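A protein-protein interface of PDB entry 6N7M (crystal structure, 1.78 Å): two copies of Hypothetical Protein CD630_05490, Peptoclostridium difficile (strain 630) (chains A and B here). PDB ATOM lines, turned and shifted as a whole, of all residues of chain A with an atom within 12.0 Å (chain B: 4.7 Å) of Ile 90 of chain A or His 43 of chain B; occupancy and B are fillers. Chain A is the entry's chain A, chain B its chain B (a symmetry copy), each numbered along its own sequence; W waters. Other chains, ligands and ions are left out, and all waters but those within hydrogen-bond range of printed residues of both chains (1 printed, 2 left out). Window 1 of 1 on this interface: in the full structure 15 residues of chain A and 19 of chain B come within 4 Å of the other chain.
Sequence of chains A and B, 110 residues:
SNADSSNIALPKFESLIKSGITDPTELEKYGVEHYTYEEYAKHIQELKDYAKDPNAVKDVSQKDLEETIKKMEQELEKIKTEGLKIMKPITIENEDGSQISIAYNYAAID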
ATOM      1  N   GLY A  31     -17.261 -18.807 -13.704  1.00  0.00           N
ATOM      2  CA  GLY A  31     -16.964 -17.528 -13.022  1.00  0.00           C
ATOM      3  C   GLY A  31     -15.924 -17.671 -11.916  1.00  0.00           C
ATOM      4  O   GLY A  31     -15.901 -18.730 -11.222  1.00  0.00           O
ATOM      5  N   VAL A  32     -15.141 -16.618 -11.702  1.00  0.00           N
ATOM      6  CA  VAL A  32     -14.123 -16.622 -10.611  1.00  0.00           C
ATOM      7  C   VAL A  32     -14.871 -16.375  -9.308  1.00  0.00           C
ATOM      8  O   VAL A  32     -15.675 -15.406  -9.266  1.00  0.00           O
ATOM      9  CB  VAL A  32     -13.024 -15.566 -10.823  1.00  0.00           C
ATOM     10  CG1 VAL A  32     -12.070 -15.513  -9.635  1.00  0.00           C
ATOM     11  CG2 VAL A  32     -12.263 -15.780 -12.118  1.00  0.00           C
ATOM     12  N   GLU A  33     -14.602 -17.206  -8.306  1.00  0.00           N
ATOM     13  CA  GLU A  33     -15.286 -17.089  -7.010  1.00  0.00           C
ATOM     14  C   GLU A  33     -14.868 -15.750  -6.424  1.00  0.00           C
ATOM     15  O   GLU A  33     -13.692 -15.516  -6.356  1.00  0.00           O
ATOM     16  CB  GLU A  33     -14.941 -18.259  -6.082  1.00  0.00           C
ATOM     17  CG  GLU A  33     -15.805 -18.307  -4.832  1.00  0.00           C
ATOM     18  CD  GLU A  33     -17.255 -18.670  -5.101  1.00  0.00           C
ATOM     19  OE1 GLU A  33     -17.496 -19.344  -6.122  1.00  0.00           O
ATOM     20  OE2 GLU A  33     -18.145 -18.256  -4.308  1.00  0.00           O
ATOM     21  N   HIS A  34     -15.821 -14.910  -6.077  1.00  0.00           N
ATOM     22  CA  HIS A  34     -15.430 -13.596  -5.532  1.00  0.00           C
ATOM     23  C   HIS A  34     -16.287 -13.244  -4.339  1.00  0.00           C
ATOM     24  O   HIS A  34     -17.319 -13.810  -4.179  1.00  0.00           O
ATOM     25  CB  HIS A  34     -15.480 -12.524  -6.608  1.00  0.00           C
ATOM     26  CG  HIS A  34     -16.817 -12.359  -7.221  1.00  0.00           C
ATOM     27  ND1 HIS A  34     -17.295 -13.199  -8.184  1.00  0.00           N
ATOM     28  CD2 HIS A  34     -17.768 -11.436  -7.022  1.00  0.00           C
ATOM     29  CE1 HIS A  34     -18.480 -12.803  -8.549  1.00  0.00           C
ATOM     30  NE2 HIS A  34     -18.780 -11.719  -7.862  1.00  0.00           N
ATOM     31  N   TYR A  35     -15.809 -12.310  -3.552  1.00  0.00           N
ATOM     32  CA  TYR A  35     -16.505 -11.878  -2.324  1.00  0.00           C
ATOM     33  C   TYR A  35     -17.767 -11.073  -2.611  1.00  0.00           C
ATOM     34  O   TYR A  35     -17.793 -10.293  -3.595  1.00  0.00           O
ATOM     35  CB  TYR A  35     -15.612 -10.948  -1.507  1.00  0.00           C
ATOM     36  CG  TYR A  35     -14.533 -11.634  -0.716  1.00  0.00           C
ATOM     37  CD1 TYR A  35     -14.838 -12.216   0.497  1.00  0.00           C
ATOM     38  CD2 TYR A  35     -13.221 -11.663  -1.153  1.00  0.00           C
ATOM     39  CE1 TYR A  35     -13.869 -12.782   1.303  1.00  0.00           C
ATOM     40  CE2 TYR A  35     -12.241 -12.259  -0.377  1.00  0.00           C
ATOM     41  CZ  TYR A  35     -12.569 -12.822   0.850  1.00  0.00           C
ATOM     42  OH  TYR A  35     -11.632 -13.407   1.637  1.00  0.00           O
ATOM     43  N   GLU A  39     -19.507 -10.334   2.826  1.00  0.00           N
ATOM     44  CA  GLU A  39     -18.409 -11.267   3.139  1.00  0.00           C
ATOM     45  C   GLU A  39     -17.100 -10.501   3.294  1.00  0.00           C
ATOM     46  O   GLU A  39     -16.352 -10.787   4.247  1.00  0.00           O
ATOM     47  CB  GLU A  39     -18.280 -12.308   2.034  1.00  0.00           C
ATOM     48  CG  GLU A  39     -19.344 -13.379   2.045  1.00  0.00           C
ATOM     49  CD  GLU A  39     -19.271 -14.315   0.841  1.00  0.00           C
ATOM     50  OE1 GLU A  39     -18.600 -13.954  -0.197  1.00  0.00           O
ATOM     51  OE2 GLU A  39     -19.880 -15.393   0.914  1.00  0.00           O
ATOM     52  N   HIS A  43     -14.648 -10.020   6.526  1.00  0.00           N
ATOM     53  CA  HIS A  43     -13.217 -10.401   6.456  1.00  0.00           C
ATOM     54  C   HIS A  43     -12.351  -9.249   6.982  1.00  0.00           C
ATOM     55  O   HIS A  43     -11.412  -9.505   7.822  1.00  0.00           O
ATOM     56  CB  HIS A  43     -12.881 -10.875   5.032  1.00  0.00           C
ATOM     57  CG  HIS A  43     -11.435 -11.102   4.814  1.00  0.00           C
ATOM     58  ND1 HIS A  43     -10.753 -12.136   5.415  1.00  0.00           N
ATOM     59  CD2 HIS A  43     -10.533 -10.433   4.078  1.00  0.00           C
ATOM     60  CE1 HIS A  43      -9.483 -12.057   5.099  1.00  0.00           C
ATOM     61  NE2 HIS A  43      -9.330 -11.043   4.267  1.00  0.00           N
ATOM     62  N   ILE A  86     -13.384  -9.287  -6.200  1.00  0.00           N
ATOM     63  CA  ILE A  86     -12.178  -9.602  -5.385  1.00  0.00           C
ATOM     64  C   ILE A  86     -12.196 -11.112  -5.229  1.00  0.00           C
ATOM     65  O   ILE A  86     -13.136 -11.621  -4.606  1.00  0.00           O
ATOM     66  CB  ILE A  86     -12.207  -8.878  -4.028  1.00  0.00           C
ATOM     67  CG1 ILE A  86     -12.297  -7.365  -4.243  1.00  0.00           C
ATOM     68  CG2 ILE A  86     -10.990  -9.262  -3.183  1.00  0.00           C
ATOM     69  CD1 ILE A  86     -12.422  -6.581  -2.970  1.00  0.00           C
ATOM     70  N   MET A  87     -11.222 -11.792  -5.829  1.00  0.00           N
ATOM     71  CA  MET A  87     -11.219 -13.262  -5.775  1.00  0.00           C
ATOM     72  C   MET A  87     -11.250 -13.762  -4.334  1.00  0.00           C
ATOM     73  O   MET A  87     -10.481 -13.260  -3.497  1.00  0.00           O
ATOM     74  CB  MET A  87     -10.004 -13.835  -6.505  1.00  0.00           C
ATOM     75  CG  MET A  87     -10.009 -15.337  -6.473  1.00  0.00           C
ATOM     76  SD  MET A  87      -8.548 -15.983  -7.570  1.00  0.00           S
ATOM     77  CE  MET A  87      -6.954 -15.073  -6.900  1.00  0.00           C
ATOM     78  N   LYS A  88     -12.132 -14.731  -4.080  1.00  0.00           N
ATOM     79  CA  LYS A  88     -12.318 -15.296  -2.715  1.00  0.00           C
ATOM     80  C   LYS A  88     -11.452 -16.540  -2.584  1.00  0.00           C
ATOM     81  O   LYS A  88     -11.307 -17.283  -3.551  1.00  0.00           O
ATOM     82  CB  LYS A  88     -13.800 -15.627  -2.508  1.00  0.00           C
ATOM     83  CG  LYS A  88     -14.245 -15.956  -1.104  1.00  0.00           C
ATOM     84  CD  LYS A  88     -15.741 -16.116  -0.986  1.00  0.00           C
ATOM     85  CE  LYS A  88     -16.206 -16.316   0.438  1.00  0.00           C
ATOM     86  NZ  LYS A  88     -15.627 -17.556   1.019  1.00  0.00           N
ATOM     87  N   PRO A  89     -10.843 -16.807  -1.408  1.00  0.00           N
ATOM     88  CA  PRO A  89     -10.075 -18.036  -1.240  1.00  0.00           C
ATOM     89  C   PRO A  89     -11.010 -19.243  -1.408  1.00  0.00           C
ATOM     90  O   PRO A  89     -12.196 -19.142  -1.088  1.00  0.00           O
ATOM     91  CB  PRO A  89      -9.546 -17.974   0.201  1.00  0.00           C
ATOM     92  CG  PRO A  89      -9.688 -16.519   0.619  1.00  0.00           C
ATOM     93  CD  PRO A  89     -10.827 -15.958  -0.207  1.00  0.00           C
ATOM     94  N   ILE A  90     -10.469 -20.347  -1.918  1.00  0.00           N
ATOM     95  CA  ILE A  90     -11.212 -21.642  -1.986  1.00  0.00           C
ATOM     96  C   ILE A  90     -10.530 -22.580  -0.979  1.00  0.00           C
ATOM     97  O   ILE A  90      -9.258 -22.606  -0.963  1.00  0.00           O
ATOM     98  CB  ILE A  90     -11.238 -22.235  -3.412  1.00  0.00           C
ATOM     99  CG1 ILE A  90     -11.914 -21.286  -4.403  1.00  0.00           C
ATOM    100  CG2 ILE A  90     -11.899 -23.605  -3.405  1.00  0.00           C
ATOM    101  CD1 ILE A  90     -12.111 -21.879  -5.796  1.00  0.00           C
ATOM    102  N   THR A  91     -11.336 -23.253  -0.146  1.00  0.00           N
ATOM    103  CA  THR A  91     -10.867 -24.235   0.876  1.00  0.00           C
ATOM    104  C   THR A  91     -10.975 -25.641   0.276  1.00  0.00           C
ATOM    105  O   THR A  91     -11.856 -25.847  -0.592  1.00  0.00           O
ATOM    106  CB  THR A  91     -11.687 -24.144   2.162  1.00  0.00           C
ATOM    107  OG1 THR A  91     -11.760 -22.781   2.572  1.00  0.00           O
ATOM    108  CG2 THR A  91     -11.127 -24.988   3.281  1.00  0.00           C
ATOM    109  N   ILE A  92     -10.164 -26.579   0.762  1.00  0.00           N
ATOM    110  CA  ILE A  92     -10.091 -27.931   0.141  1.00  0.00           C
ATOM    111  C   ILE A  92     -10.792 -28.978   1.005  1.00  0.00           C
ATOM    112  O   ILE A  92     -10.937 -30.111   0.520  1.00  0.00           O
ATOM    113  CB  ILE A  92      -8.620 -28.270  -0.130  1.00  0.00           C
ATOM    114  CG1 ILE A  92      -7.988 -27.169  -0.987  1.00  0.00           C
ATOM    115  CG2 ILE A  92      -8.485 -29.639  -0.770  1.00  0.00           C
ATOM    116  CD1 ILE A  92      -6.500 -27.167  -0.968  1.00  0.00           C
ATOM    117  N   GLU A  93     -11.230 -28.618   2.213  1.00  0.00           N
ATOM    118  CA  GLU A  93     -11.971 -29.616   3.036  1.00  0.00           C
ATOM    119  C   GLU A  93     -13.478 -29.376   2.854  1.00  0.00           C
ATOM    120  O   GLU A  93     -14.015 -29.420   1.731  1.00  0.00           O
ATOM    121  CB  GLU A  93     -11.529 -29.597   4.507  1.00  0.00           C
ATOM    122  CG  GLU A  93     -11.489 -28.223   5.164  1.00  0.00           C
ATOM    123  CD  GLU A  93     -10.226 -27.404   4.945  1.00  0.00           C
ATOM    124  OE1 GLU A  93      -9.336 -27.862   4.205  1.00  0.00           O
ATOM    125  OE2 GLU A  93     -10.129 -26.317   5.535  1.00  0.00           O
ATOM    126  N   TYR B  35       1.760 -15.787   1.412  1.00  0.00           N
ATOM    127  CA  TYR B  35       2.262 -16.968   0.691  1.00  0.00           C
ATOM    128  C   TYR B  35       3.607 -16.687   0.005  1.00  0.00           C
ATOM    129  O   TYR B  35       3.865 -15.577  -0.496  1.00  0.00           O
ATOM    130  CB  TYR B  35       1.342 -17.365  -0.460  1.00  0.00           C
ATOM    131  CG  TYR B  35       0.034 -18.019  -0.088  1.00  0.00           C
ATOM    132  CD1 TYR B  35      -0.029 -19.367   0.174  1.00  0.00           C
ATOM    133  CD2 TYR B  35      -1.146 -17.315  -0.092  1.00  0.00           C
ATOM    134  CE1 TYR B  35      -1.221 -19.997   0.473  1.00  0.00           C
ATOM    135  CE2 TYR B  35      -2.353 -17.919   0.203  1.00  0.00           C
ATOM    136  CZ  TYR B  35      -2.400 -19.277   0.454  1.00  0.00           C
ATOM    137  OH  TYR B  35      -3.563 -19.894   0.821  1.00  0.00           O
ATOM    138  N   GLU B  39       4.647 -21.966  -1.690  1.00  0.00           N
ATOM    139  CA  GLU B  39       3.409 -22.278  -0.930  1.00  0.00           C
ATOM    140  C   GLU B  39       2.190 -22.076  -1.820  1.00  0.00           C
ATOM    141  O   GLU B  39       1.278 -22.904  -1.777  1.00  0.00           O
ATOM    142  CB  GLU B  39       3.301 -21.406   0.317  1.00  0.00           C
ATOM    143  CG  GLU B  39       4.261 -21.822   1.427  1.00  0.00           C
ATOM    144  CD  GLU B  39       4.314 -20.863   2.604  1.00  0.00           C
ATOM    145  OE1 GLU B  39       4.045 -19.676   2.408  1.00  0.00           O
ATOM    146  OE2 GLU B  39       4.571 -21.319   3.728  1.00  0.00           O
ATOM    147  N   TYR B  40       2.160 -21.002  -2.597  1.00  0.00           N
ATOM    148  CA  TYR B  40       0.971 -20.732  -3.419  1.00  0.00           C
ATOM    149  C   TYR B  40       0.891 -21.743  -4.569  1.00  0.00           C
ATOM    150  O   TYR B  40      -0.241 -22.209  -4.943  1.00  0.00           O
ATOM    151  CB  TYR B  40       0.971 -19.281  -3.876  1.00  0.00           C
ATOM    152  CG  TYR B  40      -0.372 -18.794  -4.332  1.00  0.00           C
ATOM    153  CD1 TYR B  40      -1.398 -18.623  -3.408  1.00  0.00           C
ATOM    154  CD2 TYR B  40      -0.619 -18.438  -5.642  1.00  0.00           C
ATOM    155  CE1 TYR B  40      -2.644 -18.174  -3.795  1.00  0.00           C
ATOM    156  CE2 TYR B  40      -1.847 -17.955  -6.049  1.00  0.00           C
ATOM    157  CZ  TYR B  40      -2.867 -17.827  -5.121  1.00  0.00           C
ATOM    158  OH  TYR B  40      -4.080 -17.344  -5.509  1.00  0.00           O
ATOM    159  N   ALA B  41       2.050 -22.082  -5.124  1.00  0.00           N
ATOM    160  CA  ALA B  41       2.071 -23.112  -6.190  1.00  0.00           C
ATOM    161  C   ALA B  41       1.510 -24.425  -5.610  1.00  0.00           C
ATOM    162  O   ALA B  41       0.721 -25.091  -6.307  1.00  0.00           O
ATOM    163  CB  ALA B  41       3.465 -23.280  -6.721  1.00  0.00           C
ATOM    164  N   LYS B  42       1.862 -24.754  -4.363  1.00  0.00           N
ATOM    165  CA  LYS B  42       1.376 -26.009  -3.720  1.00  0.00           C
ATOM    166  C   LYS B  42      -0.138 -25.907  -3.469  1.00  0.00           C
ATOM    167  O   LYS B  42      -0.850 -26.902  -3.638  1.00  0.00           O
ATOM    168  CB  LYS B  42       2.108 -26.269  -2.402  1.00  0.00           C
ATOM    169  CG  LYS B  42       1.716 -27.562  -1.704  1.00  0.00           C
ATOM    170  CD  LYS B  42       2.357 -27.770  -0.363  1.00  0.00           C
ATOM    171  CE  LYS B  42       1.938 -29.066   0.288  1.00  0.00           C
ATOM    172  NZ  LYS B  42       2.689 -29.300   1.543  1.00  0.00           N
ATOM    173  N   HIS B  43      -0.609 -24.748  -3.038  1.00  0.00           N
ATOM    174  CA  HIS B  43      -2.061 -24.536  -2.791  1.00  0.00           C
ATOM    175  C   HIS B  43      -2.837 -24.731  -4.099  1.00  0.00           C
ATOM    176  O   HIS B  43      -3.895 -25.430  -4.069  1.00  0.00           O
ATOM    177  CB  HIS B  43      -2.283 -23.178  -2.108  1.00  0.00           C
ATOM    178  CG  HIS B  43      -3.718 -22.905  -1.833  1.00  0.00           C
ATOM    179  ND1 HIS B  43      -4.429 -21.896  -2.469  1.00  0.00           N
ATOM    180  CD2 HIS B  43      -4.596 -23.545  -1.022  1.00  0.00           C
ATOM    181  CE1 HIS B  43      -5.674 -21.919  -2.050  1.00  0.00           C
ATOM    182  NE2 HIS B  43      -5.809 -22.935  -1.185  1.00  0.00           N
ATOM    183  N   ILE B  44      -2.316 -24.215  -5.216  1.00  0.00           N
ATOM    184  CA  ILE B  44      -2.962 -24.366  -6.544  1.00  0.00           C
ATOM    185  C   ILE B  44      -3.013 -25.864  -6.910  1.00  0.00           C
ATOM    186  O   ILE B  44      -4.061 -26.315  -7.416  1.00  0.00           O
ATOM    187  CB  ILE B  44      -2.260 -23.526  -7.624  1.00  0.00           C
ATOM    188  CG1 ILE B  44      -2.547 -22.033  -7.423  1.00  0.00           C
ATOM    189  CG2 ILE B  44      -2.703 -23.961  -9.007  1.00  0.00           C
ATOM    190  CD1 ILE B  44      -1.683 -21.077  -8.228  1.00  0.00           C
ATOM    191  N   GLN B  45      -1.939 -26.603  -6.627  1.00  0.00           N
ATOM    192  CA  GLN B  45      -1.919 -28.063  -6.963  1.00  0.00           C
ATOM    193  C   GLN B  45      -2.927 -28.818  -6.077  1.00  0.00           C
ATOM    194  O   GLN B  45      -3.556 -29.780  -6.539  1.00  0.00           O
ATOM    195  CB  GLN B  45      -0.516 -28.647  -6.801  1.00  0.00           C
ATOM    196  CG  GLN B  45      -0.441 -30.140  -7.182  1.00  0.00           C
ATOM    197  CD  GLN B  45      -0.787 -30.352  -8.632  1.00  0.00           C
ATOM    198  OE1 GLN B  45      -0.401 -29.553  -9.483  1.00  0.00           O
ATOM    199  NE2 GLN B  45      -1.528 -31.424  -8.927  1.00  0.00           N
ATOM    200  N   GLU B  46      -3.058 -28.404  -4.820  1.00  0.00           N
ATOM    201  CA  GLU B  46      -4.017 -29.069  -3.900  1.00  0.00           C
ATOM    202  C   GLU B  46      -5.436 -28.797  -4.418  1.00  0.00           C
ATOM    203  O   GLU B  46      -6.279 -29.692  -4.308  1.00  0.00           O
ATOM    204  CB  GLU B  46      -3.839 -28.607  -2.455  1.00  0.00           C
ATOM    205  CG  GLU B  46      -4.445 -29.608  -1.483  1.00  0.00           C
ATOM    206  CD  GLU B  46      -4.589 -29.191  -0.031  1.00  0.00           C
ATOM    207  OE1 GLU B  46      -3.887 -28.250   0.393  1.00  0.00           O
ATOM    208  OE2 GLU B  46      -5.435 -29.801   0.665  1.00  0.00           O
ATOM    209  N   LEU B  47      -5.675 -27.620  -5.007  1.00  0.00           N
ATOM    210  CA  LEU B  47      -7.012 -27.294  -5.581  1.00  0.00           C
ATOM    211  C   LEU B  47      -7.237 -28.113  -6.850  1.00  0.00           C
ATOM    212  O   LEU B  47      -8.394 -28.477  -7.114  1.00  0.00           O
ATOM    213  CB  LEU B  47      -7.115 -25.805  -5.914  1.00  0.00           C
ATOM    214  CG  LEU B  47      -7.307 -24.887  -4.724  1.00  0.00           C
ATOM    215  CD1 LEU B  47      -7.391 -23.453  -5.213  1.00  0.00           C
ATOM    216  CD2 LEU B  47      -8.566 -25.287  -3.953  1.00  0.00           C
ATOM    217  N   VAL B  60     -18.533 -24.384  -4.716  1.00  0.00           N
ATOM    218  CA  VAL B  60     -17.953 -23.916  -6.019  1.00  0.00           C
ATOM    219  C   VAL B  60     -18.205 -24.965  -7.104  1.00  0.00           C
ATOM    220  O   VAL B  60     -17.949 -26.142  -6.855  1.00  0.00           O
ATOM    221  CB  VAL B  60     -16.461 -23.554  -5.935  1.00  0.00           C
ATOM    222  CG1 VAL B  60     -15.633 -24.738  -5.505  1.00  0.00           C
ATOM    223  CG2 VAL B  60     -15.966 -22.970  -7.234  1.00  0.00           C
ATOM    224  N   LEU B  65     -14.405 -23.509 -10.406  1.00  0.00           N
ATOM    225  CA  LEU B  65     -13.130 -23.929  -9.791  1.00  0.00           C
ATOM    226  C   LEU B  65     -12.035 -23.855 -10.853  1.00  0.00           C
ATOM    227  O   LEU B  65     -10.976 -23.306 -10.556  1.00  0.00           O
ATOM    228  CB  LEU B  65     -13.284 -25.331  -9.205  1.00  0.00           C
ATOM    229  CG  LEU B  65     -12.086 -25.871  -8.442  1.00  0.00           C
ATOM    230  CD1 LEU B  65     -11.526 -24.825  -7.487  1.00  0.00           C
ATOM    231  CD2 LEU B  65     -12.486 -27.133  -7.675  1.00  0.00           C
ATOM    232  N   THR B  68     -11.290 -20.178 -11.508  1.00  0.00           N
ATOM    233  CA  THR B  68     -10.594 -19.632 -10.313  1.00  0.00           C
ATOM    234  C   THR B  68      -9.127 -20.084 -10.315  1.00  0.00           C
ATOM    235  O   THR B  68      -8.268 -19.245 -10.057  1.00  0.00           O
ATOM    236  CB  THR B  68     -11.334 -20.009  -9.021  1.00  0.00           C
ATOM    237  OG1 THR B  68     -12.618 -19.393  -9.085  1.00  0.00           O
ATOM    238  CG2 THR B  68     -10.641 -19.506  -7.781  1.00  0.00           C
ATOM    239  N   MET B  72      -5.746 -17.847 -10.365  1.00  0.00           N
ATOM    240  CA  MET B  72      -4.682 -18.012  -9.340  1.00  0.00           C
ATOM    241  C   MET B  72      -3.321 -18.208 -10.029  1.00  0.00           C
ATOM    242  O   MET B  72      -2.339 -17.740  -9.481  1.00  0.00           O
ATOM    243  CB  MET B  72      -5.069 -19.144  -8.388  1.00  0.00           C
ATOM    244  CG  MET B  72      -6.321 -18.833  -7.615  1.00  0.00           C
ATOM    245  SD  MET B  72      -6.827 -20.433  -6.660  1.00  0.00           S
ATOM    246  CE  MET B  72      -5.439 -20.640  -5.342  1.00  0.00           C
HETATM  247  O   HOH W   1      -7.633 -29.683   3.066  1.00  0.00           O
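N of Glu 33 of chain A sits at hydrogen-bond distance from OG1 of Thr 68 of chain B (3.1 Å). NE2 of His 43 of chain B sits at hydrogen-bond distance from O of Ile 90 of chain A.
The backbone carbonyl oxygen (O) of Glu 33 of chain A lies within hydrogen-bond range of the backbone NH (N) of Lys 88 of chain A (2.9 Å). ND1 of His 34 of chain A is in hydrogen-bond range of O of Val 32 of chain A (2.9 Å).
Among the printed residues, pairs that only touch across the chains: Ile 92 of chain A with Glu 46 of chain B (2.9 Å), Ile 90 of chain A with Thr 68 of chain B (3.4 Å), Ile 90 of chain A with Leu 65 of chain B (3.4 Å), Val 32 of chain A with Thr 68 of chain B (3.5 Å), Ile 92 of chain A with Leu 47 of chain B (3.6 Å), Met 87 of chain A with Met 72 of chain B (3.6 Å), Ile 90 of chain A with Leu 47 of chain B (3.8 Å), Met 87 of chain A with Tyr 40 of chain B (3.9 Å) and Gly 31 of chain A with Thr 68 of chain B (3.97 Å).
Of the printed residues of chain B, Val 32 of chain A touches Thr 68. Of the printed residues of chain B, Met 87 of chain A touches Tyr 40 (3.9 Å) and Met 72 (3.6 Å). Of the printed residues of chain B, Ile 92 of chain A touches Glu 46 (2.9 Å) and Leu 47 (3.6 Å). Of chain A, only Met 87 (3.9 Å) comes within 4 Å of Tyr 40 of chain B. No residue of chain A comes within 4 Å of Ala 41 of chain B. No residue of chain A comes within 4 Å of Lys 42 of chain B. His 43 of chain B touches one residue of chain A. No residue of chain A comes within 4 Å of Ile 44 of chain B. Of the printed residues of chain A, Glu 46 of chain B touches Ile 92 (2.9 Å). Of chain A, only Ile 90 and Ile 92 come within 4 Å of Leu 47 of chain B. Leu 65 of chain B touches one residue of chain A. Thr 68 of chain B touches just these residues of chain A: Gly 31, Val 32, Glu 33 and Ile 90. Of the printed residues of chain A, Met 72 of chain B touches Met 87 (3.6 Å). The nearest residue of chain A that does not touch His 43 of chain B is Ile 92 of chain A (4.1 Å). The nearest printed residue of chain B that does not touch Met 87 of chain A is Thr 68 of chain B (4.1 Å).
Printed residues of chain A that touch a printed residue of chain B: Gly 31, Val 32, Glu 33, Met 87, Ile 90 and Ile 92. Hydrophobic or aromatic side chains of chain A that line the printed part of chain B: Val 32, Met 87, Ile 90 and Ile 92. Of the 14 printed residues of chain B, 7 touch a printed residue of chain A. Hydrophobic or aromatic side chains of chain B within 4 Å of the printed part of chain A: Tyr 40, His 43, Leu 47, Leu 65 and Met 72. Among the printed residues, 11 pairs touch across the chains.
Positions printed for both chains: 35, 39 and 43.
Water W1 bridges the side-chain carboxylate of Glu 93 of chain A (2.7 Å) and the side-chain carboxylate of Glu 46 of chain B (3.3 Å).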
